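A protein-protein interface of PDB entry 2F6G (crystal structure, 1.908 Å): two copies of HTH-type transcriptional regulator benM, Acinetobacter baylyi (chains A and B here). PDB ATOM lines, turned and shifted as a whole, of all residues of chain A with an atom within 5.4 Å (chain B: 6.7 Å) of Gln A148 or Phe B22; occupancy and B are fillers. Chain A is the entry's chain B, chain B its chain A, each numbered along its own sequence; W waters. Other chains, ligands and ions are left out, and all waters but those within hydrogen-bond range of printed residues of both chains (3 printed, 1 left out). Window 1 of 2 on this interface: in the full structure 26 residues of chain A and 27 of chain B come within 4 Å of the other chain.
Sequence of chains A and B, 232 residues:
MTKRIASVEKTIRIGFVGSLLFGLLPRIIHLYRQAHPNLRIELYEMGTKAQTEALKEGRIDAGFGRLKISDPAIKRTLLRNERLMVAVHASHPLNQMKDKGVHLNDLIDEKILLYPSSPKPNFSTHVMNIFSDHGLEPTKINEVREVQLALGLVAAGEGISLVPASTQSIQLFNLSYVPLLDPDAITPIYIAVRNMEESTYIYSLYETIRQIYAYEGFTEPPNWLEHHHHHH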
ATOM      1  N   GLU A 146      11.960  29.939   6.231  1.00  0.00           N
ATOM      2  CA  GLU A 146      13.032  30.915   6.042  1.00  0.00           C
ATOM      3  C   GLU A 146      12.996  31.558   4.660  1.00  0.00           C
ATOM      4  O   GLU A 146      12.302  31.087   3.759  1.00  0.00           O
ATOM      5  CB  GLU A 146      14.397  30.253   6.277  1.00  0.00           C
ATOM      6  CG  GLU A 146      14.651  29.002   5.436  1.00  0.00           C
ATOM      7  CD  GLU A 146      16.013  28.372   5.700  1.00  0.00           C
ATOM      8  OE1 GLU A 146      16.712  28.803   6.645  1.00  0.00           O
ATOM      9  OE2 GLU A 146      16.385  27.436   4.957  1.00  0.00           O
ATOM     10  N   VAL A 147      13.767  32.633   4.509  1.00  0.00           N
ATOM     11  CA  VAL A 147      13.790  33.414   3.271  1.00  0.00           C
ATOM     12  C   VAL A 147      14.167  32.604   2.023  1.00  0.00           C
ATOM     13  O   VAL A 147      13.529  32.764   0.989  1.00  0.00           O
ATOM     14  CB  VAL A 147      14.719  34.651   3.390  1.00  0.00           C
ATOM     15  CG1 VAL A 147      16.183  34.236   3.534  1.00  0.00           C
ATOM     16  CG2 VAL A 147      14.526  35.588   2.196  1.00  0.00           C
ATOM     17  N   GLN A 148      15.174  31.735   2.104  1.00  0.00           N
ATOM     18  CA  GLN A 148      15.622  31.013   0.900  1.00  0.00           C
ATOM     19  C   GLN A 148      14.609  29.962   0.454  1.00  0.00           C
ATOM     20  O   GLN A 148      14.529  29.646  -0.740  1.00  0.00           O
ATOM     21  CB  GLN A 148      17.019  30.387   1.053  1.00  0.00           C
ATOM     22  CG  GLN A 148      17.165  29.301   2.107  1.00  0.00           C
ATOM     23  CD  GLN A 148      18.072  29.715   3.242  1.00  0.00           C
ATOM     24  OE1 GLN A 148      19.095  29.073   3.507  1.00  0.00           O
ATOM     25  NE2 GLN A 148      17.710  30.800   3.917  1.00  0.00           N
ATOM     26  N   LEU A 149      13.842  29.431   1.408  1.00  0.00           N
ATOM     27  CA  LEU A 149      12.731  28.540   1.088  1.00  0.00           C
ATOM     28  C   LEU A 149      11.663  29.351   0.361  1.00  0.00           C
ATOM     29  O   LEU A 149      11.150  28.928  -0.675  1.00  0.00           O
ATOM     30  CB  LEU A 149      12.146  27.889   2.352  1.00  0.00           C
ATOM     31  CG  LEU A 149      11.669  26.431   2.267  1.00  0.00           C
ATOM     32  CD1 LEU A 149      10.707  26.108   3.416  1.00  0.00           C
ATOM     33  CD2 LEU A 149      11.018  26.093   0.930  1.00  0.00           C
ATOM     34  N   ALA A 150      11.342  30.521   0.904  1.00  0.00           N
ATOM     35  CA  ALA A 150      10.392  31.429   0.263  1.00  0.00           C
ATOM     36  C   ALA A 150      10.842  31.780  -1.155  1.00  0.00           C
ATOM     37  O   ALA A 150      10.058  31.676  -2.095  1.00  0.00           O
ATOM     38  CB  ALA A 150      10.200  32.701   1.102  1.00  0.00           C
ATOM     39  N   LEU A 151      12.106  32.173  -1.306  1.00  0.00           N
ATOM     40  CA  LEU A 151      12.656  32.522  -2.618  1.00  0.00           C
ATOM     41  C   LEU A 151      12.702  31.326  -3.568  1.00  0.00           C
ATOM     42  O   LEU A 151      12.389  31.459  -4.751  1.00  0.00           O
ATOM     43  CB  LEU A 151      14.062  33.110  -2.474  1.00  0.00           C
ATOM     44  CG  LEU A 151      14.166  34.433  -1.715  1.00  0.00           C
ATOM     45  CD1 LEU A 151      15.614  34.873  -1.611  1.00  0.00           C
ATOM     46  CD2 LEU A 151      13.319  35.516  -2.380  1.00  0.00           C
ATOM     47  N   GLY A 152      13.103  30.165  -3.047  1.00  0.00           N
ATOM     48  CA  GLY A 152      13.172  28.943  -3.842  1.00  0.00           C
ATOM     49  C   GLY A 152      11.809  28.523  -4.353  1.00  0.00           C
ATOM     50  O   GLY A 152      11.671  28.113  -5.507  1.00  0.00           O
ATOM     51  N   LEU A 153      10.798  28.648  -3.494  1.00  0.00           N
ATOM     52  CA  LEU A 153       9.420  28.357  -3.868  1.00  0.00           C
ATOM     53  C   LEU A 153       8.896  29.353  -4.901  1.00  0.00           C
ATOM     54  O   LEU A 153       8.240  28.957  -5.856  1.00  0.00           O
ATOM     55  CB  LEU A 153       8.516  28.342  -2.632  1.00  0.00           C
ATOM     56  CG  LEU A 153       8.744  27.194  -1.638  1.00  0.00           C
ATOM     57  CD1 LEU A 153       7.963  27.452  -0.349  1.00  0.00           C
ATOM     58  CD2 LEU A 153       8.368  25.845  -2.222  1.00  0.00           C
ATOM     59  N   ILE A 170      20.723  37.453  -2.912  1.00  0.00           N
ATOM     60  CA  ILE A 170      20.381  36.130  -3.442  1.00  0.00           C
ATOM     61  C   ILE A 170      19.760  36.255  -4.829  1.00  0.00           C
ATOM     62  O   ILE A 170      18.692  36.852  -4.996  1.00  0.00           O
ATOM     63  CB  ILE A 170      19.408  35.382  -2.512  1.00  0.00           C
ATOM     64  CG1 ILE A 170      19.974  35.343  -1.084  1.00  0.00           C
ATOM     65  CG2 ILE A 170      19.124  33.975  -3.050  1.00  0.00           C
ATOM     66  CD1 ILE A 170      19.109  34.615  -0.091  1.00  0.00           C
ATOM     67  N   LEU A 172      18.531  33.929  -8.091  1.00  0.00           N
ATOM     68  CA  LEU A 172      18.162  32.592  -8.533  1.00  0.00           C
ATOM     69  C   LEU A 172      17.609  32.677  -9.939  1.00  0.00           C
ATOM     70  O   LEU A 172      17.007  33.690 -10.319  1.00  0.00           O
ATOM     71  CB  LEU A 172      17.093  31.985  -7.619  1.00  0.00           C
ATOM     72  CG  LEU A 172      17.382  31.834  -6.123  1.00  0.00           C
ATOM     73  CD1 LEU A 172      16.195  31.152  -5.454  1.00  0.00           C
ATOM     74  CD2 LEU A 172      18.673  31.054  -5.855  1.00  0.00           C
ATOM     75  N   GLY B  18      17.663  21.789   1.833  1.00  0.00           N
ATOM     76  CA  GLY B  18      17.606  23.233   1.598  1.00  0.00           C
ATOM     77  C   GLY B  18      18.651  23.761   0.637  1.00  0.00           C
ATOM     78  O   GLY B  18      18.386  24.686  -0.121  1.00  0.00           O
ATOM     79  N   SER B  19      19.834  23.160   0.646  1.00  0.00           N
ATOM     80  CA  SER B  19      20.920  23.604  -0.225  1.00  0.00           C
ATOM     81  C   SER B  19      20.596  23.474  -1.720  1.00  0.00           C
ATOM     82  O   SER B  19      21.158  24.204  -2.538  1.00  0.00           O
ATOM     83  CB  SER B  19      22.212  22.855   0.103  1.00  0.00           C
ATOM     84  OG  SER B  19      22.117  21.488  -0.227  1.00  0.00           O
ATOM     85  N   LEU B  20      19.680  22.574  -2.083  1.00  0.00           N
ATOM     86  CA  LEU B  20      19.319  22.408  -3.496  1.00  0.00           C
ATOM     87  C   LEU B  20      18.484  23.573  -4.050  1.00  0.00           C
ATOM     88  O   LEU B  20      18.290  23.680  -5.259  1.00  0.00           O
ATOM     89  CB  LEU B  20      18.615  21.072  -3.720  1.00  0.00           C
ATOM     90  CG  LEU B  20      19.482  19.852  -3.388  1.00  0.00           C
ATOM     91  CD1 LEU B  20      18.702  18.557  -3.556  1.00  0.00           C
ATOM     92  CD2 LEU B  20      20.758  19.827  -4.235  1.00  0.00           C
ATOM     93  N   LEU B  21      18.014  24.457  -3.175  1.00  0.00           N
ATOM     94  CA  LEU B  21      17.234  25.619  -3.607  1.00  0.00           C
ATOM     95  C   LEU B  21      18.046  26.625  -4.407  1.00  0.00           C
ATOM     96  O   LEU B  21      17.477  27.429  -5.147  1.00  0.00           O
ATOM     97  CB  LEU B  21      16.612  26.323  -2.400  1.00  0.00           C
ATOM     98  CG  LEU B  21      15.535  25.535  -1.660  1.00  0.00           C
ATOM     99  CD1 LEU B  21      15.134  26.283  -0.414  1.00  0.00           C
ATOM    100  CD2 LEU B  21      14.330  25.268  -2.559  1.00  0.00           C
ATOM    101  N   PHE B  22      19.369  26.591  -4.251  1.00  0.00           N
ATOM    102  CA  PHE B  22      20.253  27.515  -4.968  1.00  0.00           C
ATOM    103  C   PHE B  22      20.649  26.994  -6.354  1.00  0.00           C
ATOM    104  O   PHE B  22      21.245  27.721  -7.141  1.00  0.00           O
ATOM    105  CB  PHE B  22      21.507  27.797  -4.137  1.00  0.00           C
ATOM    106  CG  PHE B  22      21.220  28.430  -2.797  1.00  0.00           C
ATOM    107  CD1 PHE B  22      20.724  29.723  -2.719  1.00  0.00           C
ATOM    108  CD2 PHE B  22      21.451  27.732  -1.618  1.00  0.00           C
ATOM    109  CE1 PHE B  22      20.462  30.319  -1.481  1.00  0.00           C
ATOM    110  CE2 PHE B  22      21.188  28.311  -0.377  1.00  0.00           C
ATOM    111  CZ  PHE B  22      20.696  29.609  -0.308  1.00  0.00           C
ATOM    112  N   GLY B  23      20.307  25.741  -6.652  1.00  0.00           N
ATOM    113  CA  GLY B  23      20.669  25.120  -7.927  1.00  0.00           C
ATOM    114  C   GLY B  23      19.495  24.946  -8.873  1.00  0.00           C
ATOM    115  O   GLY B  23      18.612  25.803  -8.950  1.00  0.00           O
ATOM    116  N   LEU B  24      19.485  23.819  -9.584  1.00  0.00           N
ATOM    117  CA  LEU B  24      18.508  23.560 -10.648  1.00  0.00           C
ATOM    118  C   LEU B  24      17.133  23.104 -10.164  1.00  0.00           C
ATOM    119  O   LEU B  24      16.202  23.029 -10.963  1.00  0.00           O
ATOM    120  CB  LEU B  24      19.051  22.489 -11.607  1.00  0.00           C
ATOM    121  CG  LEU B  24      20.053  22.902 -12.694  1.00  0.00           C
ATOM    122  CD1 LEU B  24      21.089  23.875 -12.189  1.00  0.00           C
ATOM    123  CD2 LEU B  24      20.730  21.658 -13.263  1.00  0.00           C
ATOM    124  N   LEU B  25      16.989  22.779  -8.883  1.00  0.00           N
ATOM    125  CA  LEU B  25      15.737  22.186  -8.406  1.00  0.00           C
ATOM    126  C   LEU B  25      14.500  23.047  -8.696  1.00  0.00           C
ATOM    127  O   LEU B  25      13.516  22.538  -9.228  1.00  0.00           O
ATOM    128  CB  LEU B  25      15.813  21.819  -6.915  1.00  0.00           C
ATOM    129  CG  LEU B  25      14.600  21.060  -6.354  1.00  0.00           C
ATOM    130  CD1 LEU B  25      14.219  19.872  -7.229  1.00  0.00           C
ATOM    131  CD2 LEU B  25      14.877  20.604  -4.937  1.00  0.00           C
ATOM    132  N   PRO B  26      14.538  24.352  -8.356  1.00  0.00           N
ATOM    133  CA  PRO B  26      13.375  25.200  -8.642  1.00  0.00           C
ATOM    134  C   PRO B  26      12.915  25.201 -10.106  1.00  0.00           C
ATOM    135  O   PRO B  26      11.719  25.051 -10.355  1.00  0.00           O
ATOM    136  CB  PRO B  26      13.843  26.597  -8.220  1.00  0.00           C
ATOM    137  CG  PRO B  26      14.885  26.349  -7.202  1.00  0.00           C
ATOM    138  CD  PRO B  26      15.599  25.111  -7.674  1.00  0.00           C
ATOM    139  N   GLU B  45      10.805  20.640   2.856  1.00  0.00           N
ATOM    140  CA  GLU B  45      12.223  20.778   3.151  1.00  0.00           C
ATOM    141  C   GLU B  45      12.621  19.800   4.254  1.00  0.00           C
ATOM    142  O   GLU B  45      12.103  19.878   5.366  1.00  0.00           O
ATOM    143  CB  GLU B  45      12.543  22.207   3.580  1.00  0.00           C
ATOM    144  CG  GLU B  45      14.029  22.486   3.699  1.00  0.00           C
ATOM    145  CD  GLU B  45      14.322  23.874   4.211  1.00  0.00           C
ATOM    146  OE1 GLU B  45      13.632  24.326   5.148  1.00  0.00           O
ATOM    147  OE2 GLU B  45      15.249  24.511   3.678  1.00  0.00           O
ATOM    148  N   GLU B  82      28.300  17.869  -7.804  1.00  0.00           N
ATOM    149  CA  GLU B  82      28.507  19.312  -7.792  1.00  0.00           C
ATOM    150  C   GLU B  82      29.856  19.647  -7.159  1.00  0.00           C
ATOM    151  O   GLU B  82      30.244  19.036  -6.167  1.00  0.00           O
ATOM    152  CB  GLU B  82      27.387  20.009  -7.023  1.00  0.00           C
ATOM    153  CG  GLU B  82      27.501  21.514  -7.063  1.00  0.00           C
ATOM    154  CD  GLU B  82      26.250  22.238  -6.613  1.00  0.00           C
ATOM    155  OE1 GLU B  82      25.307  21.599  -6.095  1.00  0.00           O
ATOM    156  OE2 GLU B  82      26.220  23.470  -6.781  1.00  0.00           O
ATOM    157  N   GLU B 146      23.620  27.531   9.727  1.00  0.00           N
ATOM    158  CA  GLU B 146      23.120  27.539   8.354  1.00  0.00           C
ATOM    159  C   GLU B 146      24.128  28.177   7.405  1.00  0.00           C
ATOM    160  O   GLU B 146      25.026  28.894   7.838  1.00  0.00           O
ATOM    161  CB  GLU B 146      21.790  28.307   8.292  1.00  0.00           C
ATOM    162  CG  GLU B 146      21.897  29.773   8.743  1.00  0.00           C
ATOM    163  CD  GLU B 146      20.569  30.520   8.732  1.00  0.00           C
ATOM    164  OE1 GLU B 146      19.517  29.895   8.472  1.00  0.00           O
ATOM    165  OE2 GLU B 146      20.576  31.747   8.991  1.00  0.00           O
ATOM    166  N   VAL B 147      23.958  27.921   6.111  1.00  0.00           N
ATOM    167  CA  VAL B 147      24.882  28.429   5.093  1.00  0.00           C
ATOM    168  C   VAL B 147      25.034  29.960   5.130  1.00  0.00           C
ATOM    169  O   VAL B 147      26.155  30.463   5.102  1.00  0.00           O
ATOM    170  CB  VAL B 147      24.499  27.944   3.653  1.00  0.00           C
ATOM    171  CG1 VAL B 147      23.117  28.458   3.217  1.00  0.00           C
ATOM    172  CG2 VAL B 147      25.575  28.345   2.648  1.00  0.00           C
ATOM    173  N   GLN B 148      23.930  30.700   5.216  1.00  0.00           N
ATOM    174  CA  GLN B 148      24.024  32.171   5.167  1.00  0.00           C
ATOM    175  C   GLN B 148      24.725  32.754   6.392  1.00  0.00           C
ATOM    176  O   GLN B 148      25.334  33.821   6.301  1.00  0.00           O
ATOM    177  CB  GLN B 148      22.668  32.854   4.949  1.00  0.00           C
ATOM    178  CG  GLN B 148      21.632  32.640   6.026  1.00  0.00           C
ATOM    179  CD  GLN B 148      20.501  31.760   5.563  1.00  0.00           C
ATOM    180  OE1 GLN B 148      19.342  32.182   5.537  1.00  0.00           O
ATOM    181  NE2 GLN B 148      20.828  30.533   5.172  1.00  0.00           N
ATOM    182  N   SER B 166      26.867  26.015  -6.329  1.00  0.00           N
ATOM    183  CA  SER B 166      25.611  26.738  -6.555  1.00  0.00           C
ATOM    184  C   SER B 166      25.311  27.779  -5.466  1.00  0.00           C
ATOM    185  O   SER B 166      24.411  28.594  -5.629  1.00  0.00           O
ATOM    186  CB  SER B 166      24.443  25.759  -6.688  1.00  0.00           C
ATOM    187  OG  SER B 166      24.413  24.857  -5.595  1.00  0.00           O
ATOM    188  N   THR B 167      26.079  27.761  -4.376  1.00  0.00           N
ATOM    189  CA  THR B 167      25.982  28.768  -3.313  1.00  0.00           C
ATOM    190  C   THR B 167      26.394  30.161  -3.796  1.00  0.00           C
ATOM    191  O   THR B 167      26.100  31.164  -3.134  1.00  0.00           O
ATOM    192  CB  THR B 167      26.878  28.375  -2.118  1.00  0.00           C
ATOM    193  OG1 THR B 167      26.584  27.024  -1.747  1.00  0.00           O
ATOM    194  CG2 THR B 167      26.671  29.299  -0.914  1.00  0.00           C
ATOM    195  N   GLN B 168      27.074  30.214  -4.944  1.00  0.00           N
ATOM    196  CA  GLN B 168      27.414  31.481  -5.603  1.00  0.00           C
ATOM    197  C   GLN B 168      26.186  32.321  -5.963  1.00  0.00           C
ATOM    198  O   GLN B 168      26.322  33.499  -6.310  1.00  0.00           O
ATOM    199  CB  GLN B 168      28.246  31.224  -6.857  1.00  0.00           C
ATOM    200  CG  GLN B 168      29.633  30.694  -6.551  1.00  0.00           C
ATOM    201  CD  GLN B 168      30.431  30.404  -7.798  1.00  0.00           C
ATOM    202  OE1 GLN B 168      31.267  31.206  -8.209  1.00  0.00           O
ATOM    203  NE2 GLN B 168      30.175  29.258  -8.413  1.00  0.00           N
ATOM    204  N   SER B 169      25.004  31.714  -5.887  1.00  0.00           N
ATOM    205  CA  SER B 169      23.740  32.442  -5.955  1.00  0.00           C
ATOM    206  C   SER B 169      23.683  33.531  -4.886  1.00  0.00           C
ATOM    207  O   SER B 169      23.017  34.545  -5.066  1.00  0.00           O
ATOM    208  CB  SER B 169      22.567  31.479  -5.750  1.00  0.00           C
ATOM    209  OG  SER B 169      22.503  30.520  -6.789  1.00  0.00           O
ATOM    210  N   ILE B 170      24.370  33.303  -3.765  1.00  0.00           N
ATOM    211  CA  ILE B 170      24.473  34.305  -2.704  1.00  0.00           C
ATOM    212  C   ILE B 170      25.754  35.107  -2.891  1.00  0.00           C
ATOM    213  O   ILE B 170      26.859  34.602  -2.686  1.00  0.00           O
ATOM    214  CB  ILE B 170      24.449  33.663  -1.307  1.00  0.00           C
ATOM    215  CG1 ILE B 170      23.168  32.841  -1.129  1.00  0.00           C
ATOM    216  CG2 ILE B 170      24.548  34.733  -0.204  1.00  0.00           C
ATOM    217  CD1 ILE B 170      23.236  31.832  -0.017  1.00  0.00           C
HETATM  218  O   HOH W   1      15.137  26.775   2.655  1.00  0.00           O
HETATM  219  O   HOH W   2      20.010  26.470   2.325  1.00  0.00           O
HETATM  220  O   HOH W   3      18.644  27.512   7.882  1.00  0.00           O
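OG of Ser B169 lies within hydrogen-bond range of O of Ser B166 (2.9 Å). The backbone carbonyl oxygen (O) of Phe B22 sits at hydrogen-bond distance from the side-chain hydroxyl (OG) of Ser B169. The side-chain carboxylate (OE2) of Glu A146 lies close to the side-chain amide oxygen (OE1) of Gln A148, 3.5 Å away.
Among the printed residues, merely in contact across the chains: Gln A148 with Leu B21 (3.4 Å), Ile A170 with Ser B169 (3.5 Å), Glu A146 with Glu B146 (3.5 Å), Leu A149 with Leu B21 (3.6 Å), Gly A152 with Pro B26 (3.8 Å), Leu A149 with Glu B45 (3.8 Å), Leu A172 with Leu B21 (3.9 Å), Leu A172 with Ser B169 (3.9 Å), Leu A172 with Phe B22 (3.98 Å) and Gln A148 with Phe B22 (3.997 Å).
Water W1 lies within hydrogen-bond range of the side-chain carboxylate (OE2) of Glu B45, the side-chain carboxylate (OE2) of Glu A146 and the backbone NH (N) of Leu A149. Water W3 bridges the side-chain carboxylate of Glu B146 and the side-chain carboxylate of Glu A146. Water W2 lies within hydrogen-bond range of OE1 of Gln A148 (3.0 Å) and O of Gly B18 (3.4 Å).
Printed residues of chain B that touch a printed residue of chain A: Leu B21, Phe B22, Pro B26, Glu B45, Glu B146, Gln B148 and Ser B169. Hydrophobic or aromatic side chains of chain B that line the printed part of chain A: Leu B21, Phe B22 and Pro B26. Hydrophobic or aromatic side chains of chain A that line the printed part of chain B: Leu A149 and Leu A172. Among the printed residues, no Asp or Glu carboxylate lies within 4 Å of a Lys or Arg side-chain nitrogen of the other chain.
Glu A146 touches its own counterpart, Glu B146. Gln B148 touches its own counterpart, Gln A148. Positions printed for both chains: 146, 147, 148 and 170.
Of the printed residues of chain A, Phe B22 touches Gln A148 and Leu A172. Printed residues of chain B within 4 Å of Ile A170: Ser B169. Of the printed residues of chain A, Gln B148 touches Gln A148 (2.7 Å). Printed residues of chain A within 4 Å of Glu B146: Glu A146 (3.5 Å). The nearest printed residue of chain A that does not touch Phe B22 is Ile A170 (4.2 Å). The nearest printed residue of chain A that does not touch Ser B169 is Leu A151 (8.2 Å).
The side-chain carboxylate (OE2) of Glu B45 sits close to the side-chain carboxylate (OE2) of Glu A146, at 3.4 Å. OE1 of Gln B148 lies within hydrogen-bond range of NE2 of Gln A148, at 2.7 Å.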
